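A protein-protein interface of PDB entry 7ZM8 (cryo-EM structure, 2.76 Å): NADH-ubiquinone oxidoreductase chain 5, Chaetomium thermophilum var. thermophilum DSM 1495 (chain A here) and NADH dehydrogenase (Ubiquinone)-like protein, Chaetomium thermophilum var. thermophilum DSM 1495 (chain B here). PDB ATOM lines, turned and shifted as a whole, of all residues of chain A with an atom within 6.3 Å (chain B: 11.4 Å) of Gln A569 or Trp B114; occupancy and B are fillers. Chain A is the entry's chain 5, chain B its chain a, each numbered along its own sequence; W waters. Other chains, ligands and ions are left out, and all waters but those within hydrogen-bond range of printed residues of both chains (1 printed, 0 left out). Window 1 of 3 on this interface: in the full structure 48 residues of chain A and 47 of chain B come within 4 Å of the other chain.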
ATOM      1  N   ILE A 291       7.889  23.546  -0.236  1.00  0.00           N
ATOM      2  CA  ILE A 291       8.743  24.184   0.758  1.00  0.00           C
ATOM      3  C   ILE A 291       8.232  23.915   2.165  1.00  0.00           C
ATOM      4  O   ILE A 291       9.009  23.572   3.061  1.00  0.00           O
ATOM      5  CB  ILE A 291       8.857  25.689   0.471  1.00  0.00           C
ATOM      6  CG1 ILE A 291       9.537  25.910  -0.874  1.00  0.00           C
ATOM      7  CG2 ILE A 291       9.643  26.370   1.567  1.00  0.00           C
ATOM      8  CD1 ILE A 291       9.563  27.340  -1.318  1.00  0.00           C
ATOM      9  N   GLN A 295      10.012  22.402   6.292  1.00  0.00           N
ATOM     10  CA  GLN A 295      10.296  23.439   7.269  1.00  0.00           C
ATOM     11  C   GLN A 295      10.200  22.886   8.684  1.00  0.00           C
ATOM     12  O   GLN A 295       9.445  21.953   8.957  1.00  0.00           O
ATOM     13  CB  GLN A 295       9.337  24.616   7.107  1.00  0.00           C
ATOM     14  CG  GLN A 295       9.365  25.245   5.745  1.00  0.00           C
ATOM     15  CD  GLN A 295      10.667  25.948   5.464  1.00  0.00           C
ATOM     16  OE1 GLN A 295      11.408  25.570   4.562  1.00  0.00           O
ATOM     17  NE2 GLN A 295      10.956  26.981   6.240  1.00  0.00           N
ATOM     18  N   TYR A 561      19.724  14.052   0.730  1.00  0.00           N
ATOM     19  CA  TYR A 561      20.339  15.168   1.435  1.00  0.00           C
ATOM     20  C   TYR A 561      20.198  16.450   0.630  1.00  0.00           C
ATOM     21  O   TYR A 561      19.929  17.519   1.188  1.00  0.00           O
ATOM     22  CB  TYR A 561      21.811  14.860   1.718  1.00  0.00           C
ATOM     23  CG  TYR A 561      22.595  16.002   2.320  1.00  0.00           C
ATOM     24  CD1 TYR A 561      23.209  16.947   1.513  1.00  0.00           C
ATOM     25  CD2 TYR A 561      22.730  16.130   3.695  1.00  0.00           C
ATOM     26  CE1 TYR A 561      23.920  17.982   2.053  1.00  0.00           C
ATOM     27  CE2 TYR A 561      23.442  17.163   4.240  1.00  0.00           C
ATOM     28  CZ  TYR A 561      24.039  18.084   3.416  1.00  0.00           C
ATOM     29  OH  TYR A 561      24.756  19.124   3.944  1.00  0.00           O
ATOM     30  N   ASN A 562      20.383  16.358  -0.685  1.00  0.00           N
ATOM     31  CA  ASN A 562      20.273  17.532  -1.537  1.00  0.00           C
ATOM     32  C   ASN A 562      18.821  17.935  -1.743  1.00  0.00           C
ATOM     33  O   ASN A 562      18.510  19.126  -1.832  1.00  0.00           O
ATOM     34  CB  ASN A 562      20.952  17.261  -2.875  1.00  0.00           C
ATOM     35  CG  ASN A 562      22.450  17.157  -2.749  1.00  0.00           C
ATOM     36  OD1 ASN A 562      23.154  18.160  -2.786  1.00  0.00           O
ATOM     37  ND2 ASN A 562      22.946  15.942  -2.577  1.00  0.00           N
ATOM     38  N   PHE A 564      16.397  17.467   0.409  1.00  0.00           N
ATOM     39  CA  PHE A 564      15.811  17.962   1.675  1.00  0.00           C
ATOM     40  C   PHE A 564      16.310  19.386   1.855  1.00  0.00           C
ATOM     41  O   PHE A 564      15.501  20.236   2.236  1.00  0.00           O
ATOM     42  CB  PHE A 564      16.219  17.127   2.892  1.00  0.00           C
ATOM     43  CG  PHE A 564      15.677  17.608   4.215  1.00  0.00           C
ATOM     44  CD1 PHE A 564      16.279  18.652   4.901  1.00  0.00           C
ATOM     45  CD2 PHE A 564      14.565  17.013   4.784  1.00  0.00           C
ATOM     46  CE1 PHE A 564      15.774  19.101   6.108  1.00  0.00           C
ATOM     47  CE2 PHE A 564      14.067  17.454   5.999  1.00  0.00           C
ATOM     48  CZ  PHE A 564      14.673  18.495   6.660  1.00  0.00           C
ATOM     49  N   GLY A 565      17.579  19.635   1.544  1.00  0.00           N
ATOM     50  CA  GLY A 565      18.106  20.973   1.702  1.00  0.00           C
ATOM     51  C   GLY A 565      17.647  21.929   0.625  1.00  0.00           C
ATOM     52  O   GLY A 565      17.615  23.142   0.842  1.00  0.00           O
ATOM     53  N   PHE A 566      17.287  21.406  -0.547  1.00  0.00           N
ATOM     54  CA  PHE A 566      16.795  22.263  -1.616  1.00  0.00           C
ATOM     55  C   PHE A 566      15.459  22.882  -1.243  1.00  0.00           C
ATOM     56  O   PHE A 566      15.241  24.084  -1.432  1.00  0.00           O
ATOM     57  CB  PHE A 566      16.671  21.464  -2.910  1.00  0.00           C
ATOM     58  CG  PHE A 566      16.187  22.267  -4.082  1.00  0.00           C
ATOM     59  CD1 PHE A 566      17.082  22.953  -4.882  1.00  0.00           C
ATOM     60  CD2 PHE A 566      14.837  22.325  -4.395  1.00  0.00           C
ATOM     61  CE1 PHE A 566      16.644  23.681  -5.958  1.00  0.00           C
ATOM     62  CE2 PHE A 566      14.398  23.054  -5.473  1.00  0.00           C
ATOM     63  CZ  PHE A 566      15.304  23.731  -6.255  1.00  0.00           C
ATOM     64  N   PHE A 567      14.598  22.086  -0.615  1.00  0.00           N
ATOM     65  CA  PHE A 567      13.228  22.583  -0.350  1.00  0.00           C
ATOM     66  C   PHE A 567      13.216  23.282   0.996  1.00  0.00           C
ATOM     67  O   PHE A 567      12.363  24.132   1.224  1.00  0.00           O
ATOM     68  CB  PHE A 567      12.235  21.435  -0.459  1.00  0.00           C
ATOM     69  CG  PHE A 567      11.968  20.930  -1.852  1.00  0.00           C
ATOM     70  CD1 PHE A 567      11.545  21.790  -2.851  1.00  0.00           C
ATOM     71  CD2 PHE A 567      12.108  19.587  -2.156  1.00  0.00           C
ATOM     72  CE1 PHE A 567      11.293  21.319  -4.129  1.00  0.00           C
ATOM     73  CE2 PHE A 567      11.850  19.117  -3.432  1.00  0.00           C
ATOM     74  CZ  PHE A 567      11.443  19.984  -4.416  1.00  0.00           C
ATOM     75  N   ASN A 568      14.147  22.906   1.869  1.00  0.00           N
ATOM     76  CA  ASN A 568      14.250  23.621   3.131  1.00  0.00           C
ATOM     77  C   ASN A 568      14.755  25.038   2.908  1.00  0.00           C
ATOM     78  O   ASN A 568      14.335  25.973   3.597  1.00  0.00           O
ATOM     79  CB  ASN A 568      15.164  22.858   4.086  1.00  0.00           C
ATOM     80  CG  ASN A 568      15.368  23.576   5.394  1.00  0.00           C
ATOM     81  OD1 ASN A 568      16.243  24.425   5.514  1.00  0.00           O
ATOM     82  ND2 ASN A 568      14.559  23.240   6.386  1.00  0.00           N
ATOM     83  N   GLN A 569      15.649  25.214   1.948  1.00  0.00           N
ATOM     84  CA  GLN A 569      16.203  26.511   1.618  1.00  0.00           C
ATOM     85  C   GLN A 569      15.359  27.262   0.617  1.00  0.00           C
ATOM     86  O   GLN A 569      15.841  28.229   0.019  1.00  0.00           O
ATOM     87  CB  GLN A 569      17.629  26.350   1.101  1.00  0.00           C
ATOM     88  CG  GLN A 569      18.615  25.922   2.166  1.00  0.00           C
ATOM     89  CD  GLN A 569      18.518  26.759   3.414  1.00  0.00           C
ATOM     90  OE1 GLN A 569      18.356  26.235   4.510  1.00  0.00           O
ATOM     91  NE2 GLN A 569      18.618  28.067   3.260  1.00  0.00           N
ATOM     92  N   ARG A 570      14.118  26.819   0.420  1.00  0.00           N
ATOM     93  CA  ARG A 570      13.087  27.594  -0.264  1.00  0.00           C
ATOM     94  C   ARG A 570      13.444  27.850  -1.723  1.00  0.00           C
ATOM     95  O   ARG A 570      13.296  28.967  -2.223  1.00  0.00           O
ATOM     96  CB  ARG A 570      12.822  28.907   0.470  1.00  0.00           C
ATOM     97  CG  ARG A 570      12.540  28.746   1.941  1.00  0.00           C
ATOM     98  CD  ARG A 570      12.873  30.007   2.695  1.00  0.00           C
ATOM     99  NE  ARG A 570      14.285  30.338   2.589  1.00  0.00           N
ATOM    100  CZ  ARG A 570      15.205  29.959   3.466  1.00  0.00           C
ATOM    101  NH1 ARG A 570      16.472  30.300   3.291  1.00  0.00           N
ATOM    102  NH2 ARG A 570      14.857  29.235   4.517  1.00  0.00           N
ATOM    103  N   PHE A 571      13.916  26.805  -2.404  1.00  0.00           N
ATOM    104  CA  PHE A 571      14.342  26.843  -3.800  1.00  0.00           C
ATOM    105  C   PHE A 571      15.565  27.723  -4.017  1.00  0.00           C
ATOM    106  O   PHE A 571      15.854  28.108  -5.149  1.00  0.00           O
ATOM    107  CB  PHE A 571      13.216  27.315  -4.722  1.00  0.00           C
ATOM    108  CG  PHE A 571      12.217  26.260  -5.063  1.00  0.00           C
ATOM    109  CD1 PHE A 571      11.238  25.892  -4.161  1.00  0.00           C
ATOM    110  CD2 PHE A 571      12.224  25.671  -6.305  1.00  0.00           C
ATOM    111  CE1 PHE A 571      10.299  24.938  -4.485  1.00  0.00           C
ATOM    112  CE2 PHE A 571      11.292  24.717  -6.627  1.00  0.00           C
ATOM    113  CZ  PHE A 571      10.325  24.352  -5.716  1.00  0.00           C
ATOM    114  N   LEU A 572      16.275  28.072  -2.946  1.00  0.00           N
ATOM    115  CA  LEU A 572      17.445  28.947  -2.979  1.00  0.00           C
ATOM    116  C   LEU A 572      17.134  30.327  -3.551  1.00  0.00           C
ATOM    117  O   LEU A 572      18.037  31.029  -4.003  1.00  0.00           O
ATOM    118  CB  LEU A 572      18.603  28.306  -3.750  1.00  0.00           C
ATOM    119  CG  LEU A 572      18.837  26.806  -3.563  1.00  0.00           C
ATOM    120  CD1 LEU A 572      19.921  26.333  -4.499  1.00  0.00           C
ATOM    121  CD2 LEU A 572      19.185  26.473  -2.134  1.00  0.00           C
ATOM    122  N   ILE A 573      15.864  30.732  -3.531  1.00  0.00           N
ATOM    123  CA  ILE A 573      15.478  32.031  -4.073  1.00  0.00           C
ATOM    124  C   ILE A 573      16.020  33.154  -3.201  1.00  0.00           C
ATOM    125  O   ILE A 573      16.428  34.208  -3.702  1.00  0.00           O
ATOM    126  CB  ILE A 573      13.948  32.105  -4.219  1.00  0.00           C
ATOM    127  CG1 ILE A 573      13.434  30.918  -5.030  1.00  0.00           C
ATOM    128  CG2 ILE A 573      13.523  33.412  -4.846  1.00  0.00           C
ATOM    129  CD1 ILE A 573      14.021  30.818  -6.406  1.00  0.00           C
ATOM    130  N   GLU A 574      16.022  32.954  -1.883  1.00  0.00           N
ATOM    131  CA  GLU A 574      16.651  33.913  -0.985  1.00  0.00           C
ATOM    132  C   GLU A 574      18.138  34.031  -1.271  1.00  0.00           C
ATOM    133  O   GLU A 574      18.694  35.134  -1.262  1.00  0.00           O
ATOM    134  CB  GLU A 574      16.425  33.497   0.466  1.00  0.00           C
ATOM    135  CG  GLU A 574      15.152  34.031   1.089  1.00  0.00           C
ATOM    136  CD  GLU A 574      13.950  33.155   0.806  1.00  0.00           C
ATOM    137  OE1 GLU A 574      14.025  32.313  -0.111  1.00  0.00           O
ATOM    138  OE2 GLU A 574      12.926  33.310   1.506  1.00  0.00           O
ATOM    139  N   PHE A 575      18.793  32.898  -1.528  1.00  0.00           N
ATOM    140  CA  PHE A 575      20.226  32.886  -1.790  1.00  0.00           C
ATOM    141  C   PHE A 575      20.579  33.756  -2.990  1.00  0.00           C
ATOM    142  O   PHE A 575      21.464  34.617  -2.909  1.00  0.00           O
ATOM    143  CB  PHE A 575      20.689  31.447  -2.020  1.00  0.00           C
ATOM    144  CG  PHE A 575      22.154  31.312  -2.282  1.00  0.00           C
ATOM    145  CD1 PHE A 575      23.061  32.183  -1.710  1.00  0.00           C
ATOM    146  CD2 PHE A 575      22.622  30.328  -3.126  1.00  0.00           C
ATOM    147  CE1 PHE A 575      24.405  32.061  -1.960  1.00  0.00           C
ATOM    148  CE2 PHE A 575      23.962  30.199  -3.381  1.00  0.00           C
ATOM    149  CZ  PHE A 575      24.858  31.065  -2.799  1.00  0.00           C
ATOM    150  N   GLN B  76      28.305  38.153  10.650  1.00  0.00           N
ATOM    151  CA  GLN B  76      27.472  36.999  10.962  1.00  0.00           C
ATOM    152  C   GLN B  76      28.277  35.712  11.034  1.00  0.00           C
ATOM    153  O   GLN B  76      27.752  34.701  11.507  1.00  0.00           O
ATOM    154  CB  GLN B  76      26.353  36.862   9.931  1.00  0.00           C
ATOM    155  CG  GLN B  76      26.831  36.591   8.526  1.00  0.00           C
ATOM    156  CD  GLN B  76      25.719  36.114   7.610  1.00  0.00           C
ATOM    157  OE1 GLN B  76      24.851  36.890   7.219  1.00  0.00           O
ATOM    158  NE2 GLN B  76      25.734  34.834   7.275  1.00  0.00           N
ATOM    159  N   PHE B  77      29.524  35.725  10.580  1.00  0.00           N
ATOM    160  CA  PHE B  77      30.429  34.594  10.715  1.00  0.00           C
ATOM    161  C   PHE B  77      31.323  34.699  11.938  1.00  0.00           C
ATOM    162  O   PHE B  77      32.207  33.856  12.114  1.00  0.00           O
ATOM    163  CB  PHE B  77      31.287  34.459   9.464  1.00  0.00           C
ATOM    164  CG  PHE B  77      30.488  34.303   8.210  1.00  0.00           C
ATOM    165  CD1 PHE B  77      29.654  33.220   8.042  1.00  0.00           C
ATOM    166  CD2 PHE B  77      30.563  35.247   7.206  1.00  0.00           C
ATOM    167  CE1 PHE B  77      28.924  33.078   6.904  1.00  0.00           C
ATOM    168  CE2 PHE B  77      29.830  35.106   6.063  1.00  0.00           C
ATOM    169  CZ  PHE B  77      29.010  34.020   5.910  1.00  0.00           C
ATOM    170  N   TYR B 110      21.668  39.149   4.328  1.00  0.00           N
ATOM    171  CA  TYR B 110      22.163  37.887   4.855  1.00  0.00           C
ATOM    172  C   TYR B 110      23.025  37.152   3.840  1.00  0.00           C
ATOM    173  O   TYR B 110      22.923  37.358   2.630  1.00  0.00           O
ATOM    174  CB  TYR B 110      21.016  36.984   5.279  1.00  0.00           C
ATOM    175  CG  TYR B 110      21.433  35.958   6.293  1.00  0.00           C
ATOM    176  CD1 TYR B 110      21.817  36.339   7.566  1.00  0.00           C
ATOM    177  CD2 TYR B 110      21.461  34.612   5.976  1.00  0.00           C
ATOM    178  CE1 TYR B 110      22.209  35.411   8.495  1.00  0.00           C
ATOM    179  CE2 TYR B 110      21.852  33.677   6.897  1.00  0.00           C
ATOM    180  CZ  TYR B 110      22.223  34.079   8.158  1.00  0.00           C
ATOM    181  OH  TYR B 110      22.613  33.147   9.091  1.00  0.00           O
ATOM    182  N   GLU B 111      23.882  36.283   4.354  1.00  0.00           N
ATOM    183  CA  GLU B 111      24.742  35.437   3.543  1.00  0.00           C
ATOM    184  C   GLU B 111      24.338  33.991   3.782  1.00  0.00           C
ATOM    185  O   GLU B 111      24.476  33.483   4.896  1.00  0.00           O
ATOM    186  CB  GLU B 111      26.213  35.662   3.894  1.00  0.00           C
ATOM    187  CG  GLU B 111      27.180  34.900   3.024  1.00  0.00           C
ATOM    188  CD  GLU B 111      26.769  34.898   1.571  1.00  0.00           C
ATOM    189  OE1 GLU B 111      26.857  35.964   0.928  1.00  0.00           O
ATOM    190  OE2 GLU B 111      26.354  33.832   1.069  1.00  0.00           O
ATOM    191  N   TYR B 112      23.837  33.336   2.743  1.00  0.00           N
ATOM    192  CA  TYR B 112      23.363  31.962   2.835  1.00  0.00           C
ATOM    193  C   TYR B 112      24.489  31.025   2.435  1.00  0.00           C
ATOM    194  O   TYR B 112      25.071  31.173   1.358  1.00  0.00           O
ATOM    195  CB  TYR B 112      22.136  31.750   1.953  1.00  0.00           C
ATOM    196  CG  TYR B 112      20.930  32.503   2.442  1.00  0.00           C
ATOM    197  CD1 TYR B 112      20.074  31.950   3.378  1.00  0.00           C
ATOM    198  CD2 TYR B 112      20.658  33.776   1.985  1.00  0.00           C
ATOM    199  CE1 TYR B 112      18.978  32.641   3.834  1.00  0.00           C
ATOM    200  CE2 TYR B 112      19.565  34.471   2.434  1.00  0.00           C
ATOM    201  CZ  TYR B 112      18.728  33.902   3.357  1.00  0.00           C
ATOM    202  OH  TYR B 112      17.637  34.604   3.803  1.00  0.00           O
ATOM    203  N   THR B 113      24.790  30.063   3.299  1.00  0.00           N
ATOM    204  CA  THR B 113      25.957  29.205   3.156  1.00  0.00           C
ATOM    205  C   THR B 113      25.562  27.745   2.990  1.00  0.00           C
ATOM    206  O   THR B 113      26.272  26.843   3.430  1.00  0.00           O
ATOM    207  CB  THR B 113      26.888  29.363   4.355  1.00  0.00           C
ATOM    208  OG1 THR B 113      26.215  28.928   5.542  1.00  0.00           O
ATOM    209  CG2 THR B 113      27.300  30.818   4.526  1.00  0.00           C
ATOM    210  N   TRP B 114      24.422  27.486   2.354  1.00  0.00           N
ATOM    211  CA  TRP B 114      23.980  26.104   2.208  1.00  0.00           C
ATOM    212  C   TRP B 114      24.738  25.380   1.099  1.00  0.00           C
ATOM    213  O   TRP B 114      25.290  24.300   1.326  1.00  0.00           O
ATOM    214  CB  TRP B 114      22.477  26.050   1.959  1.00  0.00           C
ATOM    215  CG  TRP B 114      22.026  24.717   1.509  1.00  0.00           C
ATOM    216  CD1 TRP B 114      21.484  24.409   0.306  1.00  0.00           C
ATOM    217  CD2 TRP B 114      22.110  23.490   2.238  1.00  0.00           C
ATOM    218  NE1 TRP B 114      21.211  23.069   0.237  1.00  0.00           N
ATOM    219  CE2 TRP B 114      21.588  22.480   1.415  1.00  0.00           C
ATOM    220  CE3 TRP B 114      22.574  23.148   3.512  1.00  0.00           C
ATOM    221  CZ2 TRP B 114      21.513  21.155   1.818  1.00  0.00           C
ATOM    222  CZ3 TRP B 114      22.498  21.831   3.908  1.00  0.00           C
ATOM    223  CH2 TRP B 114      21.966  20.854   3.066  1.00  0.00           C
ATOM    224  N   ILE B 115      24.778  25.948  -0.105  1.00  0.00           N
ATOM    225  CA  ILE B 115      25.549  25.380  -1.205  1.00  0.00           C
ATOM    226  C   ILE B 115      26.161  26.502  -2.034  1.00  0.00           C
ATOM    227  O   ILE B 115      25.963  27.687  -1.772  1.00  0.00           O
ATOM    228  CB  ILE B 115      24.722  24.429  -2.108  1.00  0.00           C
ATOM    229  CG1 ILE B 115      23.564  25.151  -2.780  1.00  0.00           C
ATOM    230  CG2 ILE B 115      24.251  23.182  -1.359  1.00  0.00           C
ATOM    231  CD1 ILE B 115      22.903  24.305  -3.825  1.00  0.00           C
ATOM    232  N   THR B 116      26.937  26.090  -3.033  1.00  0.00           N
ATOM    233  CA  THR B 116      27.669  27.001  -3.895  1.00  0.00           C
ATOM    234  C   THR B 116      26.739  27.562  -4.972  1.00  0.00           C
ATOM    235  O   THR B 116      25.769  26.907  -5.362  1.00  0.00           O
ATOM    236  CB  THR B 116      28.848  26.252  -4.527  1.00  0.00           C
ATOM    237  OG1 THR B 116      29.754  25.842  -3.495  1.00  0.00           O
ATOM    238  CG2 THR B 116      29.610  27.095  -5.539  1.00  0.00           C
ATOM    239  N   PRO B 117      26.993  28.786  -5.446  1.00  0.00           N
ATOM    240  CA  PRO B 117      26.161  29.328  -6.533  1.00  0.00           C
ATOM    241  C   PRO B 117      26.090  28.447  -7.765  1.00  0.00           C
ATOM    242  O   PRO B 117      25.020  28.334  -8.368  1.00  0.00           O
ATOM    243  CB  PRO B 117      26.839  30.666  -6.837  1.00  0.00           C
ATOM    244  CG  PRO B 117      27.381  31.086  -5.538  1.00  0.00           C
ATOM    245  CD  PRO B 117      27.779  29.843  -4.792  1.00  0.00           C
ATOM    246  N   GLY B 118      27.196  27.816  -8.159  1.00  0.00           N
ATOM    247  CA  GLY B 118      27.161  26.954  -9.329  1.00  0.00           C
ATOM    248  C   GLY B 118      26.295  25.726  -9.127  1.00  0.00           C
ATOM    249  O   GLY B 118      25.508  25.357 -10.002  1.00  0.00           O
ATOM    250  N   LYS B 119      26.427  25.076  -7.971  1.00  0.00           N
ATOM    251  CA  LYS B 119      25.601  23.909  -7.687  1.00  0.00           C
ATOM    252  C   LYS B 119      24.132  24.285  -7.578  1.00  0.00           C
ATOM    253  O   LYS B 119      23.259  23.477  -7.908  1.00  0.00           O
ATOM    254  CB  LYS B 119      26.084  23.231  -6.406  1.00  0.00           C
ATOM    255  CG  LYS B 119      25.373  21.942  -6.063  1.00  0.00           C
ATOM    256  CD  LYS B 119      25.983  21.309  -4.823  1.00  0.00           C
ATOM    257  CE  LYS B 119      25.281  20.016  -4.452  1.00  0.00           C
ATOM    258  NZ  LYS B 119      25.877  19.398  -3.236  1.00  0.00           N
ATOM    259  N   GLY B 120      23.844  25.505  -7.120  1.00  0.00           N
ATOM    260  CA  GLY B 120      22.465  25.957  -7.043  1.00  0.00           C
ATOM    261  C   GLY B 120      21.808  26.115  -8.400  1.00  0.00           C
ATOM    262  O   GLY B 120      20.659  25.715  -8.584  1.00  0.00           O
ATOM    263  N   LEU B 121      22.518  26.704  -9.368  1.00  0.00           N
ATOM    264  CA  LEU B 121      21.973  26.803 -10.718  1.00  0.00           C
ATOM    265  C   LEU B 121      21.638  25.432 -11.282  1.00  0.00           C
ATOM    266  O   LEU B 121      20.638  25.271 -11.990  1.00  0.00           O
ATOM    267  CB  LEU B 121      22.944  27.527 -11.651  1.00  0.00           C
ATOM    268  CG  LEU B 121      22.933  29.054 -11.753  1.00  0.00           C
ATOM    269  CD1 LEU B 121      21.597  29.516 -12.310  1.00  0.00           C
ATOM    270  CD2 LEU B 121      23.223  29.734 -10.447  1.00  0.00           C
ATOM    271  N   PHE B 122      22.472  24.437 -10.992  1.00  0.00           N
ATOM    272  CA  PHE B 122      22.181  23.076 -11.418  1.00  0.00           C
ATOM    273  C   PHE B 122      20.851  22.606 -10.858  1.00  0.00           C
ATOM    274  O   PHE B 122      19.970  22.171 -11.603  1.00  0.00           O
ATOM    275  CB  PHE B 122      23.321  22.158 -10.981  1.00  0.00           C
ATOM    276  CG  PHE B 122      23.163  20.733 -11.413  1.00  0.00           C
ATOM    277  CD1 PHE B 122      23.567  20.330 -12.672  1.00  0.00           C
ATOM    278  CD2 PHE B 122      22.615  19.797 -10.561  1.00  0.00           C
ATOM    279  CE1 PHE B 122      23.428  19.019 -13.072  1.00  0.00           C
ATOM    280  CE2 PHE B 122      22.478  18.483 -10.949  1.00  0.00           C
ATOM    281  CZ  PHE B 122      22.884  18.093 -12.208  1.00  0.00           C
ATOM    282  N   GLN B 123      20.666  22.734  -9.547  1.00  0.00           N
ATOM    283  CA  GLN B 123      19.460  22.215  -8.916  1.00  0.00           C
ATOM    284  C   GLN B 123      18.223  23.014  -9.305  1.00  0.00           C
ATOM    285  O   GLN B 123      17.116  22.470  -9.315  1.00  0.00           O
ATOM    286  CB  GLN B 123      19.645  22.198  -7.403  1.00  0.00           C
ATOM    287  CG  GLN B 123      20.472  21.033  -6.895  1.00  0.00           C
ATOM    288  CD  GLN B 123      20.876  21.208  -5.454  1.00  0.00           C
ATOM    289  OE1 GLN B 123      20.655  22.260  -4.868  1.00  0.00           O
ATOM    290  NE2 GLN B 123      21.470  20.180  -4.873  1.00  0.00           N
ATOM    291  N   ILE B 124      18.383  24.298  -9.624  1.00  0.00           N
ATOM    292  CA  ILE B 124      17.266  25.065 -10.169  1.00  0.00           C
ATOM    293  C   ILE B 124      16.923  24.581 -11.570  1.00  0.00           C
ATOM    294  O   ILE B 124      15.753  24.549 -11.963  1.00  0.00           O
ATOM    295  CB  ILE B 124      17.584  26.570 -10.146  1.00  0.00           C
ATOM    296  CG1 ILE B 124      17.860  27.017  -8.719  1.00  0.00           C
ATOM    297  CG2 ILE B 124      16.433  27.376 -10.719  1.00  0.00           C
ATOM    298  CD1 ILE B 124      16.691  26.805  -7.821  1.00  0.00           C
HETATM  299  O   HOH W   1      20.356  21.079  -1.797  1.00  0.00           O
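Gln A569 touches one residue of chain B. Of chain A, only Tyr A561, Gly A565, Gln A569 and Leu A572 come within 4 Å of Trp B114. Of chain B, only Trp B114 comes within 4 Å of Gly A565. No residue of chain B comes within 4 Å of Asn A568. Of chain B, only Trp B114, Ile B115 and Gly B120 come within 4 Å of Leu A572. Of the printed residues of chain B, Phe A566 touches Gln B123 and Ile B124. Of the printed residues of chain A, Pro B117 touches Phe A575. Printed residues of chain A within 4 Å of Ile B115: Leu A572 (3.7 Å) and Phe A575 (3.6 Å). Of the printed residues of chain A, Gln B123 touches Asn A562 and Phe A566. Leu B121 touches none of the printed residues of chain A. Gln A295 touches none of the printed residues of chain B. The nearest printed residue of chain B that does not touch Phe A566 is Trp B114 (4.3 Å).
Of the 16 printed residues of chain A, 10 touch a printed residue of chain B. Hydrophobic or aromatic side chains of chain A that line the printed part of chain B: Tyr A561, Phe A566, Leu A572 and Phe A575. Among the printed residues, 16 pairs touch across the chains.
Water W1 lies within hydrogen-bond range of O of Asn A562, NE1 of Trp B114, OE1 of Gln B123 and N of Phe A566.
The side-chain amide oxygen (OD1) of Asn A562 sits at hydrogen-bond distance from the side-chain amino group (NZ) of Lys B119, 3.0 Å away. OD1 of Asn A562 lies within hydrogen-bond range of NE2 of Gln B123 (3.4 Å).
The backbone carbonyl oxygen (O) of Phe A566 is in hydrogen-bond range of the backbone NH (N) of Phe A571 (3.2 Å). OD1 of Asn A568 sits close to OE1 of Gln A569 (3.0 Å). The backbone carbonyl oxygen (O) of Asn A568 sits at hydrogen-bond distance from the guanidinium group (NH2) of Arg A570, at 3.4 Å. NE2 of Gln A569 lies close to NH1 of Arg A570 (3.1 Å). NE of Arg A570 lies within salt-bridge range of OE1 of Glu A574 (3.4 Å).
Tyr A561 touches Trp B114. CA of Gly A565 touches CZ2 of Trp B114, at 3.4 Å. Ile B124 touches Phe A566. Arg A570 touches Tyr B112 (NH1 to CE1, 3.5 Å). CD1 of Ile B124 touches O of Phe A571 (3.1 Å). CD1 of Trp B114 touches CD2 of Leu A572, at 3.9 Å. Leu A572 touches Ile B115. CD1 of Leu A572 touches CA of Gly B120 (3.6 Å). Glu A574 touches Tyr B112 (CB to CZ, 3.7 Å). CZ of Phe A575 touches CG of Pro B117, 3.7 Å away.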
